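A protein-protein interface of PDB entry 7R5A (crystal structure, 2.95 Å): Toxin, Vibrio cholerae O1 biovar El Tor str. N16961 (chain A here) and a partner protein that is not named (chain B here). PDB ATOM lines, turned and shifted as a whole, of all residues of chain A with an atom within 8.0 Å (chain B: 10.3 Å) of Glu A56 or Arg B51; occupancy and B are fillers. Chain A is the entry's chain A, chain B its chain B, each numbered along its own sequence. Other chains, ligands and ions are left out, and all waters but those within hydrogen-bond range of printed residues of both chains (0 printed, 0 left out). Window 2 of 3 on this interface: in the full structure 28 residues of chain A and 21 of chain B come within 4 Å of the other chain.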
ATOM      1  N   LYS A  52     -11.212 -23.613  26.792  1.00  0.00           N
ATOM      2  CA  LYS A  52      -9.851 -24.023  27.110  1.00  0.00           C
ATOM      3  C   LYS A  52      -8.909 -23.642  25.976  1.00  0.00           C
ATOM      4  O   LYS A  52      -9.175 -23.939  24.808  1.00  0.00           O
ATOM      5  CB  LYS A  52      -9.803 -25.528  27.363  1.00  0.00           C
ATOM      6  CG  LYS A  52      -8.431 -26.057  27.739  1.00  0.00           C
ATOM      7  CD  LYS A  52      -8.479 -27.555  27.971  1.00  0.00           C
ATOM      8  CE  LYS A  52      -7.111 -28.104  28.331  1.00  0.00           C
ATOM      9  NZ  LYS A  52      -7.159 -29.575  28.547  1.00  0.00           N
ATOM     10  N   SER A  53      -7.794 -23.007  26.325  1.00  0.00           N
ATOM     11  CA  SER A  53      -6.774 -22.587  25.335  1.00  0.00           C
ATOM     12  C   SER A  53      -6.178 -23.814  24.650  1.00  0.00           C
ATOM     13  O   SER A  53      -6.008 -24.840  25.308  1.00  0.00           O
ATOM     14  CB  SER A  53      -5.690 -21.806  25.999  1.00  0.00           C
ATOM     15  OG  SER A  53      -5.679 -20.470  25.533  1.00  0.00           O
ATOM     16  N   CYS A  54      -5.839 -23.686  23.372  1.00  0.00           N
ATOM     17  CA  CYS A  54      -5.226 -24.821  22.647  1.00  0.00           C
ATOM     18  C   CYS A  54      -4.171 -24.292  21.682  1.00  0.00           C
ATOM     19  O   CYS A  54      -4.231 -24.637  20.505  1.00  0.00           O
ATOM     20  CB  CYS A  54      -6.269 -25.617  21.883  1.00  0.00           C
ATOM     21  SG  CYS A  54      -7.179 -24.616  20.689  1.00  0.00           S
ATOM     22  N   ASP A  55      -3.174 -23.571  22.203  1.00  0.00           N
ATOM     23  CA  ASP A  55      -2.056 -23.005  21.397  1.00  0.00           C
ATOM     24  C   ASP A  55      -1.237 -24.132  20.765  1.00  0.00           C
ATOM     25  O   ASP A  55      -0.695 -23.921  19.691  1.00  0.00           O
ATOM     26  CB  ASP A  55      -1.181 -22.079  22.236  1.00  0.00           C
ATOM     27  CG  ASP A  55      -1.901 -20.813  22.640  1.00  0.00           C
ATOM     28  OD1 ASP A  55      -3.107 -20.734  22.406  1.00  0.00           O
ATOM     29  OD2 ASP A  55      -1.246 -19.921  23.178  1.00  0.00           O
ATOM     30  N   GLU A  56      -1.125 -25.273  21.442  1.00  0.00           N
ATOM     31  CA  GLU A  56      -0.438 -26.469  20.913  1.00  0.00           C
ATOM     32  C   GLU A  56      -0.955 -26.737  19.500  1.00  0.00           C
ATOM     33  O   GLU A  56      -0.141 -26.835  18.580  1.00  0.00           O
ATOM     34  CB  GLU A  56      -0.776 -27.647  21.823  1.00  0.00           C
ATOM     35  CG  GLU A  56      -0.708 -27.290  23.297  1.00  0.00           C
ATOM     36  CD  GLU A  56      -2.036 -27.069  24.003  1.00  0.00           C
ATOM     37  OE1 GLU A  56      -2.938 -27.899  23.828  1.00  0.00           O
ATOM     38  OE2 GLU A  56      -2.153 -26.074  24.742  1.00  0.00           O
ATOM     39  N   ILE A  57      -2.272 -26.846  19.344  1.00  0.00           N
ATOM     40  CA  ILE A  57      -2.864 -27.113  18.004  1.00  0.00           C
ATOM     41  C   ILE A  57      -2.532 -25.951  17.067  1.00  0.00           C
ATOM     42  O   ILE A  57      -1.936 -26.202  16.021  1.00  0.00           O
ATOM     43  CB  ILE A  57      -4.375 -27.346  18.138  1.00  0.00           C
ATOM     44  CG1 ILE A  57      -4.662 -28.664  18.851  1.00  0.00           C
ATOM     45  CG2 ILE A  57      -5.039 -27.298  16.780  1.00  0.00           C
ATOM     46  CD1 ILE A  57      -6.028 -28.725  19.474  1.00  0.00           C
ATOM     47  N   ARG A  58      -2.921 -24.731  17.430  1.00  0.00           N
ATOM     48  CA  ARG A  58      -2.636 -23.540  16.592  1.00  0.00           C
ATOM     49  C   ARG A  58      -2.490 -22.355  17.535  1.00  0.00           C
ATOM     50  O   ARG A  58      -3.243 -22.289  18.494  1.00  0.00           O
ATOM     51  CB  ARG A  58      -3.762 -23.289  15.591  1.00  0.00           C
ATOM     52  N   GLU A  59      -1.558 -21.456  17.258  1.00  0.00           N
ATOM     53  CA  GLU A  59      -1.311 -20.345  18.205  1.00  0.00           C
ATOM     54  C   GLU A  59      -2.469 -19.350  18.244  1.00  0.00           C
ATOM     55  O   GLU A  59      -2.735 -18.718  17.223  1.00  0.00           O
ATOM     56  CB  GLU A  59      -0.010 -19.631  17.850  1.00  0.00           C
ATOM     57  CG  GLU A  59       0.550 -18.823  18.997  1.00  0.00           C
ATOM     58  CD  GLU A  59       1.148 -19.688  20.087  1.00  0.00           C
ATOM     59  OE1 GLU A  59       1.716 -20.739  19.745  1.00  0.00           O
ATOM     60  OE2 GLU A  59       1.039 -19.309  21.269  1.00  0.00           O
ATOM     61  N   GLY A  60      -3.102 -19.214  19.409  1.00  0.00           N
ATOM     62  CA  GLY A  60      -4.154 -18.205  19.611  1.00  0.00           C
ATOM     63  C   GLY A  60      -5.548 -18.780  19.674  1.00  0.00           C
ATOM     64  O   GLY A  60      -6.435 -18.067  20.141  1.00  0.00           O
ATOM     65  N   TYR A  61      -5.736 -20.027  19.254  1.00  0.00           N
ATOM     66  CA  TYR A  61      -7.099 -20.608  19.218  1.00  0.00           C
ATOM     67  C   TYR A  61      -7.525 -21.135  20.585  1.00  0.00           C
ATOM     68  O   TYR A  61      -6.676 -21.473  21.396  1.00  0.00           O
ATOM     69  CB  TYR A  61      -7.162 -21.752  18.210  1.00  0.00           C
ATOM     70  CG  TYR A  61      -7.144 -21.308  16.775  1.00  0.00           C
ATOM     71  CD1 TYR A  61      -8.269 -21.381  15.983  1.00  0.00           C
ATOM     72  CD2 TYR A  61      -5.993 -20.804  16.214  1.00  0.00           C
ATOM     73  CE1 TYR A  61      -8.248 -20.959  14.665  1.00  0.00           C
ATOM     74  CE2 TYR A  61      -5.951 -20.382  14.899  1.00  0.00           C
ATOM     75  CZ  TYR A  61      -7.084 -20.461  14.120  1.00  0.00           C
ATOM     76  OH  TYR A  61      -7.025 -20.041  12.827  1.00  0.00           O
ATOM     77  N   LYS A  63     -10.918 -23.702  22.259  1.00  0.00           N
ATOM     78  CA  LYS A  63     -11.956 -24.639  21.862  1.00  0.00           C
ATOM     79  C   LYS A  63     -12.995 -24.782  22.965  1.00  0.00           C
ATOM     80  O   LYS A  63     -12.681 -24.714  24.157  1.00  0.00           O
ATOM     81  CB  LYS A  63     -11.367 -26.010  21.503  1.00  0.00           C
ATOM     82  CG  LYS A  63     -10.472 -26.625  22.560  1.00  0.00           C
ATOM     83  CD  LYS A  63      -9.803 -27.866  22.004  1.00  0.00           C
ATOM     84  CE  LYS A  63      -9.024 -28.624  23.061  1.00  0.00           C
ATOM     85  NZ  LYS A  63      -8.419 -29.858  22.485  1.00  0.00           N
ATOM     86  N   PHE A  72     -14.180 -24.013  17.494  1.00  0.00           N
ATOM     87  CA  PHE A  72     -12.852 -23.420  17.552  1.00  0.00           C
ATOM     88  C   PHE A  72     -12.971 -21.934  17.251  1.00  0.00           C
ATOM     89  O   PHE A  72     -13.579 -21.547  16.245  1.00  0.00           O
ATOM     90  CB  PHE A  72     -11.900 -24.099  16.565  1.00  0.00           C
ATOM     91  CG  PHE A  72     -11.515 -25.499  16.961  1.00  0.00           C
ATOM     92  CD1 PHE A  72     -12.330 -26.574  16.643  1.00  0.00           C
ATOM     93  CD2 PHE A  72     -10.340 -25.737  17.657  1.00  0.00           C
ATOM     94  CE1 PHE A  72     -11.977 -27.861  17.008  1.00  0.00           C
ATOM     95  CE2 PHE A  72      -9.983 -27.021  18.024  1.00  0.00           C
ATOM     96  CZ  PHE A  72     -10.803 -28.084  17.700  1.00  0.00           C
ATOM     97  N   ARG A  85     -14.232 -22.688  13.071  1.00  0.00           N
ATOM     98  CA  ARG A  85     -14.624 -24.037  12.693  1.00  0.00           C
ATOM     99  C   ARG A  85     -15.549 -24.623  13.749  1.00  0.00           C
ATOM    100  O   ARG A  85     -15.444 -24.306  14.937  1.00  0.00           O
ATOM    101  CB  ARG A  85     -13.399 -24.944  12.512  1.00  0.00           C
ATOM    102  CG  ARG A  85     -12.748 -24.853  11.144  1.00  0.00           C
ATOM    103  CD  ARG A  85     -13.705 -25.337  10.074  1.00  0.00           C
ATOM    104  NE  ARG A  85     -13.015 -25.767   8.863  1.00  0.00           N
ATOM    105  CZ  ARG A  85     -13.606 -26.418   7.869  1.00  0.00           C
ATOM    106  NH1 ARG A  85     -14.896 -26.715   7.949  1.00  0.00           N
ATOM    107  NH2 ARG A  85     -12.911 -26.777   6.799  1.00  0.00           N
ATOM    108  N   LEU A  87     -16.285 -28.351  14.193  1.00  0.00           N
ATOM    109  CA  LEU A  87     -16.066 -29.769  13.750  1.00  0.00           C
ATOM    110  C   LEU A  87     -16.766 -30.721  14.676  1.00  0.00           C
ATOM    111  O   LEU A  87     -17.386 -30.282  15.635  1.00  0.00           O
ATOM    112  CB  LEU A  87     -14.569 -29.940  13.587  1.00  0.00           C
ATOM    113  CG  LEU A  87     -13.885 -28.810  12.838  1.00  0.00           C
ATOM    114  CD1 LEU A  87     -12.441 -28.674  13.257  1.00  0.00           C
ATOM    115  CD2 LEU A  87     -13.978 -29.055  11.354  1.00  0.00           C
ATOM    116  N   ASP A  92      -8.061 -33.693  19.225  1.00  0.00           N
ATOM    117  CA  ASP A  92      -7.097 -34.362  20.139  1.00  0.00           C
ATOM    118  C   ASP A  92      -6.663 -33.375  21.229  1.00  0.00           C
ATOM    119  O   ASP A  92      -6.558 -32.170  20.926  1.00  0.00           O
ATOM    120  CB  ASP A  92      -5.897 -34.922  19.371  1.00  0.00           C
ATOM    121  CG  ASP A  92      -5.262 -33.914  18.429  1.00  0.00           C
ATOM    122  OD1 ASP A  92      -5.698 -32.746  18.441  1.00  0.00           O
ATOM    123  OD2 ASP A  92      -4.335 -34.305  17.691  1.00  0.00           O
ATOM    124  N   VAL A  93      -6.426 -33.877  22.445  1.00  0.00           N
ATOM    125  CA  VAL A  93      -5.996 -33.016  23.587  1.00  0.00           C
ATOM    126  C   VAL A  93      -4.515 -32.661  23.408  1.00  0.00           C
ATOM    127  O   VAL A  93      -4.205 -31.458  23.301  1.00  0.00           O
ATOM    128  CB  VAL A  93      -6.247 -33.710  24.941  1.00  0.00           C
ATOM    129  CG1 VAL A  93      -5.983 -32.776  26.112  1.00  0.00           C
ATOM    130  CG2 VAL A  93      -7.648 -34.294  25.024  1.00  0.00           C
ATOM    131  N   ASN A  94      -3.646 -33.676  23.376  1.00  0.00           N
ATOM    132  CA  ASN A  94      -2.183 -33.463  23.203  1.00  0.00           C
ATOM    133  C   ASN A  94      -1.452 -32.618  24.253  1.00  0.00           C
ATOM    134  O   ASN A  94      -0.561 -31.835  23.865  1.00  0.00           O
ATOM    135  CB  ASN A  94      -1.839 -33.021  21.778  1.00  0.00           C
ATOM    136  N   PRO A  95      -1.782 -32.742  25.558  1.00  0.00           N
ATOM    137  CA  PRO A  95      -1.330 -31.812  26.596  1.00  0.00           C
ATOM    138  C   PRO A  95       0.201 -31.797  26.711  1.00  0.00           C
ATOM    139  O   PRO A  95       0.675 -31.293  27.713  1.00  0.00           O
ATOM    140  CB  PRO A  95      -1.948 -32.396  27.874  1.00  0.00           C
ATOM    141  CG  PRO A  95      -2.017 -33.880  27.598  1.00  0.00           C
ATOM    142  CD  PRO A  95      -2.319 -33.986  26.117  1.00  0.00           C
ATOM    143  N   GLN B  43      -2.379 -40.286  15.255  1.00  0.00           N
ATOM    144  CA  GLN B  43      -2.727 -39.069  15.981  1.00  0.00           C
ATOM    145  C   GLN B  43      -2.030 -37.848  15.395  1.00  0.00           C
ATOM    146  O   GLN B  43      -2.613 -36.760  15.367  1.00  0.00           O
ATOM    147  CB  GLN B  43      -2.386 -39.208  17.466  1.00  0.00           C
ATOM    148  CG  GLN B  43      -3.022 -38.133  18.333  1.00  0.00           C
ATOM    149  CD  GLN B  43      -2.569 -38.197  19.778  1.00  0.00           C
ATOM    150  OE1 GLN B  43      -1.390 -38.408  20.064  1.00  0.00           O
ATOM    151  NE2 GLN B  43      -3.507 -38.011  20.699  1.00  0.00           N
ATOM    152  N   GLU B  44      -0.791 -38.007  14.920  1.00  0.00           N
ATOM    153  CA  GLU B  44      -0.099 -36.884  14.290  1.00  0.00           C
ATOM    154  C   GLU B  44      -0.788 -36.464  12.995  1.00  0.00           C
ATOM    155  O   GLU B  44      -0.946 -35.263  12.728  1.00  0.00           O
ATOM    156  CB  GLU B  44       1.364 -37.250  14.033  1.00  0.00           C
ATOM    157  CG  GLU B  44       2.189 -36.138  13.393  1.00  0.00           C
ATOM    158  CD  GLU B  44       2.439 -34.965  14.328  1.00  0.00           C
ATOM    159  OE1 GLU B  44       2.284 -35.134  15.557  1.00  0.00           O
ATOM    160  OE2 GLU B  44       2.793 -33.872  13.836  1.00  0.00           O
ATOM    161  N   THR B  45      -1.200 -37.435  12.176  1.00  0.00           N
ATOM    162  CA  THR B  45      -1.937 -37.102  10.958  1.00  0.00           C
ATOM    163  C   THR B  45      -3.266 -36.436  11.291  1.00  0.00           C
ATOM    164  O   THR B  45      -3.694 -35.504  10.601  1.00  0.00           O
ATOM    165  CB  THR B  45      -2.167 -38.353  10.110  1.00  0.00           C
ATOM    166  OG1 THR B  45      -2.950 -39.299  10.847  1.00  0.00           O
ATOM    167  CG2 THR B  45      -0.843 -38.987   9.723  1.00  0.00           C
ATOM    168  N   LYS B  46      -3.928 -36.898  12.354  1.00  0.00           N
ATOM    169  CA  LYS B  46      -5.166 -36.270  12.802  1.00  0.00           C
ATOM    170  C   LYS B  46      -4.928 -34.826  13.227  1.00  0.00           C
ATOM    171  O   LYS B  46      -5.727 -33.933  12.915  1.00  0.00           O
ATOM    172  CB  LYS B  46      -5.752 -37.089  13.951  1.00  0.00           C
ATOM    173  CG  LYS B  46      -7.100 -36.636  14.465  1.00  0.00           C
ATOM    174  CD  LYS B  46      -7.683 -37.706  15.382  1.00  0.00           C
ATOM    175  CE  LYS B  46      -9.068 -37.336  15.874  1.00  0.00           C
ATOM    176  NZ  LYS B  46      -9.786 -38.506  16.449  1.00  0.00           N
ATOM    177  N   LEU B  47      -3.827 -34.583  13.941  1.00  0.00           N
ATOM    178  CA  LEU B  47      -3.475 -33.231  14.361  1.00  0.00           C
ATOM    179  C   LEU B  47      -3.244 -32.328  13.158  1.00  0.00           C
ATOM    180  O   LEU B  47      -3.743 -31.196  13.108  1.00  0.00           O
ATOM    181  CB  LEU B  47      -2.228 -33.280  15.243  1.00  0.00           C
ATOM    182  CG  LEU B  47      -1.663 -31.944  15.719  1.00  0.00           C
ATOM    183  CD1 LEU B  47      -2.652 -31.248  16.642  1.00  0.00           C
ATOM    184  CD2 LEU B  47      -0.313 -32.149  16.403  1.00  0.00           C
ATOM    185  N   GLN B  48      -2.482 -32.813  12.176  1.00  0.00           N
ATOM    186  CA  GLN B  48      -2.228 -32.007  10.987  1.00  0.00           C
ATOM    187  C   GLN B  48      -3.504 -31.769  10.186  1.00  0.00           C
ATOM    188  O   GLN B  48      -3.672 -30.696   9.594  1.00  0.00           O
ATOM    189  CB  GLN B  48      -1.160 -32.668  10.116  1.00  0.00           C
ATOM    190  CG  GLN B  48       0.257 -32.562  10.674  1.00  0.00           C
ATOM    191  CD  GLN B  48       0.773 -31.132  10.721  1.00  0.00           C
ATOM    192  OE1 GLN B  48       1.577 -30.781  11.586  1.00  0.00           O
ATOM    193  NE2 GLN B  48       0.322 -30.303   9.784  1.00  0.00           N
ATOM    194  N   SER B  49      -4.420 -32.740  10.173  1.00  0.00           N
ATOM    195  CA  SER B  49      -5.690 -32.544   9.482  1.00  0.00           C
ATOM    196  C   SER B  49      -6.537 -31.483  10.176  1.00  0.00           C
ATOM    197  O   SER B  49      -7.148 -30.637   9.513  1.00  0.00           O
ATOM    198  CB  SER B  49      -6.447 -33.867   9.398  1.00  0.00           C
ATOM    199  OG  SER B  49      -5.616 -34.881   8.865  1.00  0.00           O
ATOM    200  N   LEU B  50      -6.585 -31.516  11.509  1.00  0.00           N
ATOM    201  CA  LEU B  50      -7.287 -30.470  12.249  1.00  0.00           C
ATOM    202  C   LEU B  50      -6.663 -29.106  11.984  1.00  0.00           C
ATOM    203  O   LEU B  50      -7.374 -28.102  11.830  1.00  0.00           O
ATOM    204  CB  LEU B  50      -7.269 -30.786  13.745  1.00  0.00           C
ATOM    205  CG  LEU B  50      -8.191 -29.952  14.639  1.00  0.00           C
ATOM    206  CD1 LEU B  50      -9.628 -30.430  14.513  1.00  0.00           C
ATOM    207  CD2 LEU B  50      -7.733 -29.993  16.090  1.00  0.00           C
ATOM    208  N   ARG B  51      -5.330 -29.054  11.916  1.00  0.00           N
ATOM    209  CA  ARG B  51      -4.650 -27.793  11.640  1.00  0.00           C
ATOM    210  C   ARG B  51      -5.002 -27.262  10.256  1.00  0.00           C
ATOM    211  O   ARG B  51      -5.251 -26.062  10.090  1.00  0.00           O
ATOM    212  CB  ARG B  51      -3.137 -27.964  11.779  1.00  0.00           C
ATOM    213  CG  ARG B  51      -2.645 -28.019  13.215  1.00  0.00           C
ATOM    214  CD  ARG B  51      -1.224 -27.490  13.323  1.00  0.00           C
ATOM    215  NE  ARG B  51      -0.215 -28.538  13.193  1.00  0.00           N
ATOM    216  CZ  ARG B  51       0.473 -29.040  14.214  1.00  0.00           C
ATOM    217  NH1 ARG B  51       0.264 -28.588  15.443  1.00  0.00           N
ATOM    218  NH2 ARG B  51       1.375 -29.990  14.006  1.00  0.00           N
ATOM    219  N   GLN B  52      -5.030 -28.137   9.246  1.00  0.00           N
ATOM    220  CA  GLN B  52      -5.372 -27.668   7.906  1.00  0.00           C
ATOM    221  C   GLN B  52      -6.841 -27.269   7.816  1.00  0.00           C
ATOM    222  O   GLN B  52      -7.185 -26.356   7.055  1.00  0.00           O
ATOM    223  CB  GLN B  52      -5.032 -28.726   6.854  1.00  0.00           C
ATOM    224  N   LEU B  53      -7.715 -27.921   8.589  1.00  0.00           N
ATOM    225  CA  LEU B  53      -9.108 -27.490   8.654  1.00  0.00           C
ATOM    226  C   LEU B  53      -9.212 -26.081   9.222  1.00  0.00           C
ATOM    227  O   LEU B  53      -9.933 -25.231   8.685  1.00  0.00           O
ATOM    228  CB  LEU B  53      -9.924 -28.467   9.500  1.00  0.00           C
ATOM    229  CG  LEU B  53     -10.265 -29.822   8.884  1.00  0.00           C
ATOM    230  CD1 LEU B  53     -11.001 -30.685   9.895  1.00  0.00           C
ATOM    231  CD2 LEU B  53     -11.096 -29.642   7.625  1.00  0.00           C
ATOM    232  N   LEU B  54      -8.486 -25.816  10.311  1.00  0.00           N
ATOM    233  CA  LEU B  54      -8.492 -24.474  10.888  1.00  0.00           C
ATOM    234  C   LEU B  54      -7.913 -23.450   9.919  1.00  0.00           C
ATOM    235  O   LEU B  54      -8.410 -22.321   9.828  1.00  0.00           O
ATOM    236  CB  LEU B  54      -7.718 -24.464  12.206  1.00  0.00           C
ATOM    237  CG  LEU B  54      -8.328 -25.292  13.339  1.00  0.00           C
ATOM    238  CD1 LEU B  54      -7.441 -25.252  14.571  1.00  0.00           C
ATOM    239  CD2 LEU B  54      -9.729 -24.802  13.669  1.00  0.00           C
ATOM    240  N   ILE B  55      -6.867 -23.827   9.181  1.00  0.00           N
ATOM    241  CA  ILE B  55      -6.265 -22.913   8.209  1.00  0.00           C
ATOM    242  C   ILE B  55      -7.267 -22.561   7.117  1.00  0.00           C
ATOM    243  O   ILE B  55      -7.520 -21.381   6.832  1.00  0.00           O
ATOM    244  CB  ILE B  55      -4.981 -23.527   7.620  1.00  0.00           C
ATOM    245  CG1 ILE B  55      -3.868 -23.568   8.668  1.00  0.00           C
ATOM    246  CG2 ILE B  55      -4.530 -22.751   6.390  1.00  0.00           C
ATOM    247  CD1 ILE B  55      -3.320 -22.208   9.039  1.00  0.00           C
ATOM    248  N   GLU B  56      -7.850 -23.584   6.481  1.00  0.00           N
ATOM    249  CA  GLU B  56      -8.820 -23.358   5.418  1.00  0.00           C
ATOM    250  C   GLU B  56     -10.081 -22.667   5.918  1.00  0.00           C
ATOM    251  O   GLU B  56     -10.796 -22.057   5.115  1.00  0.00           O
ATOM    252  CB  GLU B  56      -9.181 -24.684   4.745  1.00  0.00           C
ATOM    253  CG  GLU B  56      -8.024 -25.324   3.998  1.00  0.00           C
ATOM    254  CD  GLU B  56      -8.402 -26.645   3.356  1.00  0.00           C
ATOM    255  OE1 GLU B  56      -9.491 -27.171   3.666  1.00  0.00           O
ATOM    256  OE2 GLU B  56      -7.607 -27.155   2.538  1.00  0.00           O
ATOM    257  N   GLY B  57     -10.372 -22.747   7.214  1.00  0.00           N
ATOM    258  CA  GLY B  57     -11.494 -22.015   7.762  1.00  0.00           C
ATOM    259  C   GLY B  57     -11.175 -20.560   8.026  1.00  0.00           C
ATOM    260  O   GLY B  57     -12.025 -19.686   7.826  1.00  0.00           O
ATOM    261  N   GLU B  58      -9.949 -20.280   8.471  1.00  0.00           N
ATOM    262  CA  GLU B  58      -9.595 -18.912   8.828  1.00  0.00           C
ATOM    263  C   GLU B  58      -9.231 -18.070   7.613  1.00  0.00           C
ATOM    264  O   GLU B  58      -9.470 -16.857   7.618  1.00  0.00           O
ATOM    265  CB  GLU B  58      -8.444 -18.900   9.838  1.00  0.00           C
ATOM    266  CG  GLU B  58      -7.098 -19.349   9.294  1.00  0.00           C
ATOM    267  CD  GLU B  58      -5.970 -19.110  10.280  1.00  0.00           C
ATOM    268  OE1 GLU B  58      -6.221 -18.469  11.322  1.00  0.00           O
ATOM    269  OE2 GLU B  58      -4.837 -19.562  10.019  1.00  0.00           O
ATOM    270  N   GLN B  59      -8.660 -18.672   6.570  1.00  0.00           N
ATOM    271  CA  GLN B  59      -8.343 -17.912   5.367  1.00  0.00           C
ATOM    272  C   GLN B  59      -9.514 -17.844   4.394  1.00  0.00           C
ATOM    273  O   GLN B  59      -9.340 -17.381   3.263  1.00  0.00           O
ATOM    274  CB  GLN B  59      -7.101 -18.485   4.675  1.00  0.00           C
ATOM    275  CG  GLN B  59      -7.269 -19.843   4.023  1.00  0.00           C
ATOM    276  CD  GLN B  59      -5.971 -20.340   3.412  1.00  0.00           C
ATOM    277  OE1 GLN B  59      -4.904 -19.769   3.647  1.00  0.00           O
ATOM    278  NE2 GLN B  59      -6.055 -21.403   2.622  1.00  0.00           N
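NH1 of Arg B51 sits close to O of Ile A57, 3.3 Å away. OH of Tyr A61 sits close to OE1 of Glu B58. NE of Arg A85 sits at hydrogen-bond distance from O of Leu B53 (3.1 Å).
The side-chain amide oxygen of Gln B48 lies within hydrogen-bond range of the guanidinium group of Arg B51, 2.6 Å away. N of Phe A72 is in hydrogen-bond range of O of Arg A85, at 2.9 Å. The backbone NH of Cys A54 lies within hydrogen-bond range of the backbone carbonyl oxygen of Tyr A61 (3.1 Å). The side-chain amino group (NZ) of Lys A63 is in hydrogen-bond range of the backbone carbonyl oxygen (O) of Asp A92, 3.4 Å away.
Glu A56 touches Arg B51 (O to NH1, 3.6 Å). Leu B47 touches Ile A57. CD2 of Leu B50 touches CG2 of Ile A57, at 3.9 Å. CZ of Phe A72 touches CD2 of Leu B50, 3.96 Å away. Phe A72 touches Leu B54. CD2 of Leu B54 touches CB of Arg A85 (3.9 Å). Leu B50 touches Leu A87. CD1 of Leu B53 touches CD2 of Leu A87 (3.7 Å). Asp A92 touches Gln B43 (OD2 to O, 3.8 Å). Leu B47 touches Asp A92 (CB to OD2, 3.4 Å).
No residue of chain B comes within 4 Å of Cys A54. Asp A55 touches none of the printed residues of chain B. Glu A56 touches just one residue of chain B: Arg B51 (3.6 Å). Of the printed residues of chain B, Ile A57 touches Leu B47 (3.9 Å), Leu B50 (3.9 Å), Arg B51 (3.1 Å) and Leu B54 (3.9 Å). Of the printed residues of chain B, Tyr A61 touches Glu B58 (2.3 Å). Printed residues of chain B within 4 Å of Arg A85: Leu B53 and Leu B54. No residue of chain B comes within 4 Å of Asn A94. Printed residues of chain A within 4 Å of Gln B43: Asp A92. Of the printed residues of chain A, Leu B50 touches Ile A57, Phe A72 and Leu A87. Printed residues of chain A within 4 Å of Glu B58: Tyr A61. The nearest residue of chain A that does not touch Arg B51 is Arg A58 (5.2 Å).
Hydrophobic or aromatic side chains of chain B that line the printed part of chain A: Leu B47, Leu B50, Leu B53 and Leu B54. Among the printed residues, 14 pairs touch across the chains. Among the printed residues, no Asp or Glu carboxylate lies within 4 Å of a Lys or Arg side-chain nitrogen of the other chain.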
